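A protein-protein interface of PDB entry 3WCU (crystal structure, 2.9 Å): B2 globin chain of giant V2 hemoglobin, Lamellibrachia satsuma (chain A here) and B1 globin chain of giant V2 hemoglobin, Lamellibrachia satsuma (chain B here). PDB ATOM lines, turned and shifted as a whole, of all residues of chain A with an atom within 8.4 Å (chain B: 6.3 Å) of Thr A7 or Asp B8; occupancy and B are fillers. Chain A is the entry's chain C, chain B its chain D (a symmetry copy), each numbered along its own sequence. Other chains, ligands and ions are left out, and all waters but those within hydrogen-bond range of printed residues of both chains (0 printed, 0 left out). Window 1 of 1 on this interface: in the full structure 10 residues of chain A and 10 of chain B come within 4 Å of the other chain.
O of Cys A5 sits at hydrogen-bond distance from ND2 of Asn B135 (3.3 Å). The guanidinium group (NH2) of Arg A10 is in salt-bridge range of the side-chain carboxylate (OD1) of Asp B131, 2.5 Å away. The side-chain carboxylate of Asp B8 lies within hydrogen-bond range of the side-chain hydroxyl of Thr A7. The side-chain carboxylate (OE2) of Glu A8 lies within hydrogen-bond range of the backbone NH (N) of Ala B7 (3.5 Å). OE1 of Glu A8 sits at hydrogen-bond distance from OG of Ser B5, at 2.9 Å.
Of the 17 printed residues of chain B, 8 touch a printed residue of chain A. Printed residues of chain B that touch a printed residue of chain A: Ser B5, Glu B6, Ala B7, Asp B8, Ile B11, Asn B129, Asp B131 and Asn B135. Of the 16 printed residues of chain A, 7 touch a printed residue of chain B.
Thr A7 touches just these residues of chain B: Ala B7, Asp B8 and Ile B11. Asp B8 touches just these residues of chain A: Thr A6 and Thr A7. Ala B7 touches just these residues of chain A: Thr A7 and Glu A8. No residue of chain A comes within 4 Å of Ala B9. Printed residues of chain B within 4 Å of Arg A10: Asp B131. Printed residues of chain B within 4 Å of Pro A85: Asn B129 and Asp B131. Printed residues of chain A within 4 Å of Ser B5: Thr A6 and Glu A8. Of the printed residues of chain A, Asp B131 touches Arg A10 (2.5 Å) and Pro A85 (3.0 Å). Of the printed residues of chain A, Ile B11 touches Thr A7. Arg A11 touches none of the printed residues of chain B. Leu B82 touches none of the printed residues of chain A. The nearest residue of chain B that does not touch Thr A7 is Ser B5 (4.3 Å).
Among the printed residues, merely in contact across the chains: Pro A85 with Asp B131 (3.0 Å), Pro A85 with Asn B129 (3.2 Å), Thr A7 with Ile B11 (3.3 Å), Thr A6 with Ser B5 (3.3 Å), Thr A6 with Asp B8 (3.5 Å), Ser A4 with Asn B135 (3.8 Å), Glu A8 with Glu B6 (3.8 Å) and Thr A7 with Ala B7 (3.9 Å).
O of Leu A82 is in hydrogen-bond range of NH1 of Arg A10 (2.7 Å). SG of Cys A136 forms a disulfide with SG of Cys A5, 2.0 Å away. The backbone carbonyl oxygen (O) of Cys A5 lies within hydrogen-bond range of the guanidinium group (NE) of Arg A10. The backbone carbonyl oxygen of Glu B6 lies within hydrogen-bond range of the side-chain hydroxyl of Thr B10, at 2.4 Å. The side-chain sulfur (SG) of Cys B136 forms a disulfide with the side-chain sulfur (SG) of Cys B4. The side-chain hydroxyl (OG) of Ser A2 sits close to the backbone NH (N) of Ser A4 (3.1 Å).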
ATOM      1  N   SER A   2     -22.576 -10.606 -23.707  1.00  0.00           N
ATOM      2  CA  SER A   2     -23.864 -11.075 -23.207  1.00  0.00           C
ATOM      3  C   SER A   2     -24.904  -9.960 -23.044  1.00  0.00           C
ATOM      4  O   SER A   2     -26.100 -10.172 -23.284  1.00  0.00           O
ATOM      5  CB  SER A   2     -23.659 -11.784 -21.866  1.00  0.00           C
ATOM      6  OG  SER A   2     -24.795 -11.635 -21.037  1.00  0.00           O
ATOM      7  N   SER A   4     -25.823  -8.755 -20.322  1.00  0.00           N
ATOM      8  CA  SER A   4     -26.487  -8.964 -19.037  1.00  0.00           C
ATOM      9  C   SER A   4     -25.990  -7.981 -18.002  1.00  0.00           C
ATOM     10  O   SER A   4     -24.836  -7.575 -18.052  1.00  0.00           O
ATOM     11  CB  SER A   4     -26.208 -10.365 -18.513  1.00  0.00           C
ATOM     12  OG  SER A   4     -26.471 -11.339 -19.496  1.00  0.00           O
ATOM     13  N   CYS A   5     -26.857  -7.612 -17.062  1.00  0.00           N
ATOM     14  CA  CYS A   5     -26.492  -6.693 -15.990  1.00  0.00           C
ATOM     15  C   CYS A   5     -25.880  -7.540 -14.879  1.00  0.00           C
ATOM     16  O   CYS A   5     -26.586  -8.066 -14.029  1.00  0.00           O
ATOM     17  CB  CYS A   5     -27.732  -5.953 -15.476  1.00  0.00           C
ATOM     18  SG  CYS A   5     -27.546  -5.056 -13.896  1.00  0.00           S
ATOM     19  N   THR A   6     -24.557  -7.668 -14.898  1.00  0.00           N
ATOM     20  CA  THR A   6     -23.827  -8.470 -13.926  1.00  0.00           C
ATOM     21  C   THR A   6     -23.703  -7.839 -12.546  1.00  0.00           C
ATOM     22  O   THR A   6     -23.809  -6.619 -12.389  1.00  0.00           O
ATOM     23  CB  THR A   6     -22.424  -8.747 -14.422  1.00  0.00           C
ATOM     24  OG1 THR A   6     -21.690  -7.514 -14.460  1.00  0.00           O
ATOM     25  CG2 THR A   6     -22.477  -9.371 -15.816  1.00  0.00           C
ATOM     26  N   THR A   7     -23.453  -8.685 -11.549  1.00  0.00           N
ATOM     27  CA  THR A   7     -23.311  -8.229 -10.176  1.00  0.00           C
ATOM     28  C   THR A   7     -22.321  -7.079 -10.061  1.00  0.00           C
ATOM     29  O   THR A   7     -22.519  -6.176  -9.257  1.00  0.00           O
ATOM     30  CB  THR A   7     -22.864  -9.367  -9.249  1.00  0.00           C
ATOM     31  OG1 THR A   7     -23.809 -10.440  -9.328  1.00  0.00           O
ATOM     32  CG2 THR A   7     -22.789  -8.877  -7.810  1.00  0.00           C
ATOM     33  N   GLU A   8     -21.254  -7.105 -10.853  1.00  0.00           N
ATOM     34  CA  GLU A   8     -20.294  -6.018 -10.800  1.00  0.00           C
ATOM     35  C   GLU A   8     -20.981  -4.759 -11.329  1.00  0.00           C
ATOM     36  O   GLU A   8     -20.953  -3.712 -10.669  1.00  0.00           O
ATOM     37  CB  GLU A   8     -19.027  -6.329 -11.612  1.00  0.00           C
ATOM     38  CG  GLU A   8     -19.098  -7.513 -12.560  1.00  0.00           C
ATOM     39  CD  GLU A   8     -18.979  -8.853 -11.853  1.00  0.00           C
ATOM     40  OE1 GLU A   8     -19.938  -9.231 -11.153  1.00  0.00           O
ATOM     41  OE2 GLU A   8     -17.931  -9.531 -11.989  1.00  0.00           O
ATOM     42  N   ASP A   9     -21.615  -4.861 -12.499  1.00  0.00           N
ATOM     43  CA  ASP A   9     -22.321  -3.715 -13.069  1.00  0.00           C
ATOM     44  C   ASP A   9     -23.247  -3.117 -12.033  1.00  0.00           C
ATOM     45  O   ASP A   9     -23.337  -1.901 -11.909  1.00  0.00           O
ATOM     46  CB  ASP A   9     -23.131  -4.120 -14.287  1.00  0.00           C
ATOM     47  CG  ASP A   9     -22.263  -4.579 -15.419  1.00  0.00           C
ATOM     48  OD1 ASP A   9     -21.071  -4.201 -15.436  1.00  0.00           O
ATOM     49  OD2 ASP A   9     -22.767  -5.308 -16.295  1.00  0.00           O
ATOM     50  N   ARG A  10     -23.935  -3.980 -11.291  1.00  0.00           N
ATOM     51  CA  ARG A  10     -24.837  -3.542 -10.234  1.00  0.00           C
ATOM     52  C   ARG A  10     -24.117  -2.726  -9.143  1.00  0.00           C
ATOM     53  O   ARG A  10     -24.512  -1.596  -8.844  1.00  0.00           O
ATOM     54  CB  ARG A  10     -25.528  -4.759  -9.608  1.00  0.00           C
ATOM     55  CG  ARG A  10     -26.455  -5.482 -10.564  1.00  0.00           C
ATOM     56  CD  ARG A  10     -26.808  -6.888 -10.093  1.00  0.00           C
ATOM     57  NE  ARG A  10     -27.661  -7.582 -11.063  1.00  0.00           N
ATOM     58  CZ  ARG A  10     -28.992  -7.554 -11.055  1.00  0.00           C
ATOM     59  NH1 ARG A  10     -29.637  -6.867 -10.116  1.00  0.00           N
ATOM     60  NH2 ARG A  10     -29.680  -8.206 -11.992  1.00  0.00           N
ATOM     61  N   ARG A  11     -23.063  -3.285  -8.548  1.00  0.00           N
ATOM     62  CA  ARG A  11     -22.324  -2.573  -7.498  1.00  0.00           C
ATOM     63  C   ARG A  11     -21.819  -1.196  -7.997  1.00  0.00           C
ATOM     64  O   ARG A  11     -21.839  -0.190  -7.273  1.00  0.00           O
ATOM     65  CB  ARG A  11     -21.128  -3.414  -7.012  1.00  0.00           C
ATOM     66  CG  ARG A  11     -21.459  -4.778  -6.410  1.00  0.00           C
ATOM     67  CD  ARG A  11     -20.172  -5.516  -6.006  1.00  0.00           C
ATOM     68  NE  ARG A  11     -20.356  -6.937  -5.681  1.00  0.00           N
ATOM     69  CZ  ARG A  11     -20.998  -7.403  -4.606  1.00  0.00           C
ATOM     70  NH1 ARG A  11     -21.099  -8.711  -4.416  1.00  0.00           N
ATOM     71  NH2 ARG A  11     -21.541  -6.574  -3.718  1.00  0.00           N
ATOM     72  N   GLU A  12     -21.366  -1.164  -9.240  1.00  0.00           N
ATOM     73  CA  GLU A  12     -20.864   0.060  -9.812  1.00  0.00           C
ATOM     74  C   GLU A  12     -21.982   1.083 -10.021  1.00  0.00           C
ATOM     75  O   GLU A  12     -21.903   2.212  -9.525  1.00  0.00           O
ATOM     76  CB  GLU A  12     -20.193  -0.262 -11.121  1.00  0.00           C
ATOM     77  CG  GLU A  12     -19.405   0.843 -11.694  1.00  0.00           C
ATOM     78  CD  GLU A  12     -18.757   0.392 -12.961  1.00  0.00           C
ATOM     79  OE1 GLU A  12     -18.022   1.181 -13.584  1.00  0.00           O
ATOM     80  OE2 GLU A  12     -18.988  -0.777 -13.337  1.00  0.00           O
ATOM     81  N   MET A  13     -23.025   0.711 -10.758  1.00  0.00           N
ATOM     82  CA  MET A  13     -24.124   1.642 -10.964  1.00  0.00           C
ATOM     83  C   MET A  13     -24.656   2.139  -9.612  1.00  0.00           C
ATOM     84  O   MET A  13     -24.860   3.343  -9.408  1.00  0.00           O
ATOM     85  CB  MET A  13     -25.271   0.982 -11.735  1.00  0.00           C
ATOM     86  CG  MET A  13     -26.534   1.850 -11.807  1.00  0.00           C
ATOM     87  SD  MET A  13     -27.992   0.988 -12.433  1.00  0.00           S
ATOM     88  CE  MET A  13     -28.481   2.092 -13.733  1.00  0.00           C
ATOM     89  N   GLN A  14     -24.876   1.206  -8.693  1.00  0.00           N
ATOM     90  CA  GLN A  14     -25.413   1.549  -7.384  1.00  0.00           C
ATOM     91  C   GLN A  14     -24.591   2.627  -6.694  1.00  0.00           C
ATOM     92  O   GLN A  14     -25.137   3.567  -6.099  1.00  0.00           O
ATOM     93  CB  GLN A  14     -25.473   0.302  -6.517  1.00  0.00           C
ATOM     94  CG  GLN A  14     -26.854  -0.095  -6.094  1.00  0.00           C
ATOM     95  CD  GLN A  14     -26.915  -1.556  -5.683  1.00  0.00           C
ATOM     96  OE1 GLN A  14     -27.864  -1.989  -5.022  1.00  0.00           O
ATOM     97  NE2 GLN A  14     -25.905  -2.330  -6.082  1.00  0.00           N
ATOM     98  N   LEU A  82     -31.633  -3.740  -7.334  1.00  0.00           N
ATOM     99  CA  LEU A  82     -30.761  -4.614  -8.109  1.00  0.00           C
ATOM    100  C   LEU A  82     -30.046  -5.523  -7.103  1.00  0.00           C
ATOM    101  O   LEU A  82     -29.505  -6.570  -7.454  1.00  0.00           O
ATOM    102  CB  LEU A  82     -29.754  -3.779  -8.900  1.00  0.00           C
ATOM    103  CG  LEU A  82     -30.303  -3.106 -10.160  1.00  0.00           C
ATOM    104  CD1 LEU A  82     -29.381  -2.036 -10.698  1.00  0.00           C
ATOM    105  CD2 LEU A  82     -30.502  -4.173 -11.201  1.00  0.00           C
ATOM    106  N   SER A  83     -30.071  -5.112  -5.837  1.00  0.00           N
ATOM    107  CA  SER A  83     -29.452  -5.869  -4.758  1.00  0.00           C
ATOM    108  C   SER A  83     -30.322  -7.024  -4.285  1.00  0.00           C
ATOM    109  O   SER A  83     -29.828  -7.934  -3.628  1.00  0.00           O
ATOM    110  CB  SER A  83     -29.138  -4.951  -3.572  1.00  0.00           C
ATOM    111  OG  SER A  83     -27.936  -4.229  -3.783  1.00  0.00           O
ATOM    112  N   PRO A  85     -32.961  -8.924  -6.465  1.00  0.00           N
ATOM    113  CA  PRO A  85     -33.753  -9.238  -7.655  1.00  0.00           C
ATOM    114  C   PRO A  85     -35.145  -9.860  -7.463  1.00  0.00           C
ATOM    115  O   PRO A  85     -36.081  -9.467  -8.158  1.00  0.00           O
ATOM    116  CB  PRO A  85     -32.797 -10.098  -8.507  1.00  0.00           C
ATOM    117  CG  PRO A  85     -31.705 -10.516  -7.560  1.00  0.00           C
ATOM    118  CD  PRO A  85     -31.561  -9.335  -6.656  1.00  0.00           C
ATOM    119  N   CYS A 136     -27.663  -2.172 -17.218  1.00  0.00           N
ATOM    120  CA  CYS A 136     -28.576  -2.302 -16.091  1.00  0.00           C
ATOM    121  C   CYS A 136     -29.776  -1.367 -16.174  1.00  0.00           C
ATOM    122  O   CYS A 136     -30.794  -1.599 -15.515  1.00  0.00           O
ATOM    123  CB  CYS A 136     -27.853  -2.091 -14.761  1.00  0.00           C
ATOM    124  SG  CYS A 136     -26.579  -3.333 -14.382  1.00  0.00           S
ATOM    125  N   CYS B   4     -21.248 -15.910 -17.859  1.00  0.00           N
ATOM    126  CA  CYS B   4     -21.679 -14.916 -16.893  1.00  0.00           C
ATOM    127  C   CYS B   4     -20.471 -14.344 -16.173  1.00  0.00           C
ATOM    128  O   CYS B   4     -19.445 -15.017 -16.037  1.00  0.00           O
ATOM    129  CB  CYS B   4     -22.719 -15.505 -15.893  1.00  0.00           C
ATOM    130  SG  CYS B   4     -22.317 -17.033 -14.946  1.00  0.00           S
ATOM    131  N   SER B   5     -20.594 -13.095 -15.730  1.00  0.00           N
ATOM    132  CA  SER B   5     -19.511 -12.449 -15.019  1.00  0.00           C
ATOM    133  C   SER B   5     -19.081 -13.323 -13.843  1.00  0.00           C
ATOM    134  O   SER B   5     -19.837 -14.161 -13.359  1.00  0.00           O
ATOM    135  CB  SER B   5     -19.965 -11.110 -14.501  1.00  0.00           C
ATOM    136  OG  SER B   5     -20.456 -11.280 -13.192  1.00  0.00           O
ATOM    137  N   GLU B   6     -17.867 -13.114 -13.364  1.00  0.00           N
ATOM    138  CA  GLU B   6     -17.357 -13.923 -12.268  1.00  0.00           C
ATOM    139  C   GLU B   6     -18.131 -13.844 -10.958  1.00  0.00           C
ATOM    140  O   GLU B   6     -18.418 -14.872 -10.346  1.00  0.00           O
ATOM    141  CB  GLU B   6     -15.902 -13.573 -12.006  1.00  0.00           C
ATOM    142  CG  GLU B   6     -15.359 -14.265 -10.801  1.00  0.00           C
ATOM    143  CD  GLU B   6     -14.016 -13.731 -10.411  1.00  0.00           C
ATOM    144  OE1 GLU B   6     -13.073 -13.877 -11.217  1.00  0.00           O
ATOM    145  OE2 GLU B   6     -13.905 -13.158  -9.303  1.00  0.00           O
ATOM    146  N   ALA B   7     -18.450 -12.630 -10.526  1.00  0.00           N
ATOM    147  CA  ALA B   7     -19.164 -12.448  -9.271  1.00  0.00           C
ATOM    148  C   ALA B   7     -20.540 -13.098  -9.351  1.00  0.00           C
ATOM    149  O   ALA B   7     -21.144 -13.463  -8.328  1.00  0.00           O
ATOM    150  CB  ALA B   7     -19.287 -10.959  -8.944  1.00  0.00           C
ATOM    151  N   ASP B   8     -21.034 -13.234 -10.575  1.00  0.00           N
ATOM    152  CA  ASP B   8     -22.321 -13.866 -10.794  1.00  0.00           C
ATOM    153  C   ASP B   8     -22.140 -15.359 -10.522  1.00  0.00           C
ATOM    154  O   ASP B   8     -22.688 -15.889  -9.554  1.00  0.00           O
ATOM    155  CB  ASP B   8     -22.790 -13.632 -12.237  1.00  0.00           C
ATOM    156  CG  ASP B   8     -23.570 -12.330 -12.405  1.00  0.00           C
ATOM    157  OD1 ASP B   8     -23.755 -11.905 -13.564  1.00  0.00           O
ATOM    158  OD2 ASP B   8     -24.010 -11.740 -11.392  1.00  0.00           O
ATOM    159  N   ALA B   9     -21.358 -16.025 -11.371  1.00  0.00           N
ATOM    160  CA  ALA B   9     -21.099 -17.455 -11.229  1.00  0.00           C
ATOM    161  C   ALA B   9     -20.912 -17.770  -9.756  1.00  0.00           C
ATOM    162  O   ALA B   9     -21.328 -18.822  -9.264  1.00  0.00           O
ATOM    163  CB  ALA B   9     -19.841 -17.858 -12.015  1.00  0.00           C
ATOM    164  N   THR B  10     -20.294 -16.830  -9.055  1.00  0.00           N
ATOM    165  CA  THR B  10     -20.039 -16.984  -7.635  1.00  0.00           C
ATOM    166  C   THR B  10     -21.328 -17.128  -6.821  1.00  0.00           C
ATOM    167  O   THR B  10     -21.491 -18.095  -6.070  1.00  0.00           O
ATOM    168  CB  THR B  10     -19.220 -15.795  -7.117  1.00  0.00           C
ATOM    169  OG1 THR B  10     -18.126 -15.566  -8.019  1.00  0.00           O
ATOM    170  CG2 THR B  10     -18.679 -16.078  -5.713  1.00  0.00           C
ATOM    171  N   ILE B  11     -22.242 -16.174  -6.973  1.00  0.00           N
ATOM    172  CA  ILE B  11     -23.500 -16.219  -6.247  1.00  0.00           C
ATOM    173  C   ILE B  11     -24.254 -17.504  -6.554  1.00  0.00           C
ATOM    174  O   ILE B  11     -24.835 -18.145  -5.664  1.00  0.00           O
ATOM    175  CB  ILE B  11     -24.375 -15.042  -6.617  1.00  0.00           C
ATOM    176  CG1 ILE B  11     -23.637 -13.750  -6.267  1.00  0.00           C
ATOM    177  CG2 ILE B  11     -25.717 -15.140  -5.874  1.00  0.00           C
ATOM    178  CD1 ILE B  11     -24.287 -12.482  -6.796  1.00  0.00           C
ATOM    179  N   VAL B  12     -24.227 -17.882  -7.824  1.00  0.00           N
ATOM    180  CA  VAL B  12     -24.909 -19.079  -8.250  1.00  0.00           C
ATOM    181  C   VAL B  12     -24.258 -20.325  -7.681  1.00  0.00           C
ATOM    182  O   VAL B  12     -24.934 -21.165  -7.107  1.00  0.00           O
ATOM    183  CB  VAL B  12     -24.954 -19.182  -9.785  1.00  0.00           C
ATOM    184  CG1 VAL B  12     -25.612 -20.478 -10.195  1.00  0.00           C
ATOM    185  CG2 VAL B  12     -25.709 -18.002 -10.363  1.00  0.00           C
ATOM    186  N   ILE B  13     -22.946 -20.449  -7.820  1.00  0.00           N
ATOM    187  CA  ILE B  13     -22.255 -21.634  -7.318  1.00  0.00           C
ATOM    188  C   ILE B  13     -22.352 -21.854  -5.805  1.00  0.00           C
ATOM    189  O   ILE B  13     -22.230 -22.983  -5.311  1.00  0.00           O
ATOM    190  CB  ILE B  13     -20.781 -21.585  -7.707  1.00  0.00           C
ATOM    191  CG1 ILE B  13     -20.670 -21.603  -9.230  1.00  0.00           C
ATOM    192  CG2 ILE B  13     -20.019 -22.736  -7.049  1.00  0.00           C
ATOM    193  CD1 ILE B  13     -19.244 -21.560  -9.743  1.00  0.00           C
ATOM    194  N   LEU B  82     -18.662 -22.841 -14.072  1.00  0.00           N
ATOM    195  CA  LEU B  82     -19.025 -21.551 -14.623  1.00  0.00           C
ATOM    196  C   LEU B  82     -17.836 -20.616 -14.750  1.00  0.00           C
ATOM    197  O   LEU B  82     -17.816 -19.762 -15.624  1.00  0.00           O
ATOM    198  CB  LEU B  82     -20.102 -20.905 -13.755  1.00  0.00           C
ATOM    199  CG  LEU B  82     -21.523 -21.254 -14.192  1.00  0.00           C
ATOM    200  CD1 LEU B  82     -22.555 -20.834 -13.144  1.00  0.00           C
ATOM    201  CD2 LEU B  82     -21.784 -20.564 -15.518  1.00  0.00           C
ATOM    202  N   ASN B 129     -31.141 -15.789  -5.652  1.00  0.00           N
ATOM    203  CA  ASN B 129     -31.006 -14.606  -6.495  1.00  0.00           C
ATOM    204  C   ASN B 129     -31.392 -14.882  -7.950  1.00  0.00           C
ATOM    205  O   ASN B 129     -30.595 -15.407  -8.732  1.00  0.00           O
ATOM    206  CB  ASN B 129     -29.571 -14.077  -6.443  1.00  0.00           C
ATOM    207  CG  ASN B 129     -29.365 -12.877  -7.333  1.00  0.00           C
ATOM    208  OD1 ASN B 129     -29.774 -12.865  -8.490  1.00  0.00           O
ATOM    209  ND2 ASN B 129     -28.720 -11.861  -6.799  1.00  0.00           N
ATOM    210  N   ASP B 131     -31.699 -12.952 -10.610  1.00  0.00           N
ATOM    211  CA  ASP B 131     -30.866 -12.297 -11.620  1.00  0.00           C
ATOM    212  C   ASP B 131     -29.528 -12.981 -11.891  1.00  0.00           C
ATOM    213  O   ASP B 131     -29.206 -13.301 -13.043  1.00  0.00           O
ATOM    214  CB  ASP B 131     -30.636 -10.837 -11.234  1.00  0.00           C
ATOM    215  CG  ASP B 131     -31.877  -9.988 -11.415  1.00  0.00           C
ATOM    216  OD1 ASP B 131     -31.855  -8.817 -10.992  1.00  0.00           O
ATOM    217  OD2 ASP B 131     -32.871 -10.496 -11.987  1.00  0.00           O
ATOM    218  N   ALA B 132     -28.750 -13.198 -10.834  1.00  0.00           N
ATOM    219  CA  ALA B 132     -27.455 -13.856 -10.969  1.00  0.00           C
ATOM    220  C   ALA B 132     -27.679 -15.179 -11.691  1.00  0.00           C
ATOM    221  O   ALA B 132     -26.966 -15.493 -12.647  1.00  0.00           O
ATOM    222  CB  ALA B 132     -26.819 -14.090  -9.580  1.00  0.00           C
ATOM    223  N   TRP B 133     -28.680 -15.945 -11.244  1.00  0.00           N
ATOM    224  CA  TRP B 133     -28.989 -17.228 -11.873  1.00  0.00           C
ATOM    225  C   TRP B 133     -29.400 -17.072 -13.328  1.00  0.00           C
ATOM    226  O   TRP B 133     -28.936 -17.816 -14.194  1.00  0.00           O
ATOM    227  CB  TRP B 133     -30.094 -17.958 -11.131  1.00  0.00           C
ATOM    228  CG  TRP B 133     -29.624 -18.689  -9.924  1.00  0.00           C
ATOM    229  CD1 TRP B 133     -29.452 -18.185  -8.663  1.00  0.00           C
ATOM    230  CD2 TRP B 133     -29.272 -20.069  -9.853  1.00  0.00           C
ATOM    231  NE1 TRP B 133     -29.016 -19.173  -7.811  1.00  0.00           N
ATOM    232  CE2 TRP B 133     -28.896 -20.338  -8.516  1.00  0.00           C
ATOM    233  CE3 TRP B 133     -29.237 -21.107 -10.789  1.00  0.00           C
ATOM    234  CZ2 TRP B 133     -28.487 -21.600  -8.093  1.00  0.00           C
ATOM    235  CZ3 TRP B 133     -28.826 -22.369 -10.369  1.00  0.00           C
ATOM    236  CH2 TRP B 133     -28.458 -22.603  -9.032  1.00  0.00           C
ATOM    237  N   ASN B 135     -28.592 -14.745 -15.483  1.00  0.00           N
ATOM    238  CA  ASN B 135     -27.398 -14.447 -16.278  1.00  0.00           C
ATOM    239  C   ASN B 135     -26.491 -15.663 -16.442  1.00  0.00           C
ATOM    240  O   ASN B 135     -25.785 -15.779 -17.448  1.00  0.00           O
ATOM    241  CB  ASN B 135     -26.559 -13.325 -15.662  1.00  0.00           C
ATOM    242  CG  ASN B 135     -27.382 -12.123 -15.223  1.00  0.00           C
ATOM    243  OD1 ASN B 135     -28.451 -11.835 -15.769  1.00  0.00           O
ATOM    244  ND2 ASN B 135     -26.861 -11.397 -14.233  1.00  0.00           N
ATOM    245  N   CYS B 136     -26.476 -16.557 -15.454  1.00  0.00           N
ATOM    246  CA  CYS B 136     -25.637 -17.751 -15.558  1.00  0.00           C
ATOM    247  C   CYS B 136     -26.366 -18.941 -16.164  1.00  0.00           C
ATOM    248  O   CYS B 136     -25.812 -19.645 -17.004  1.00  0.00           O
ATOM    249  CB  CYS B 136     -25.084 -18.173 -14.197  1.00  0.00           C
ATOM    250  SG  CYS B 136     -23.750 -17.144 -13.505  1.00  0.00           S
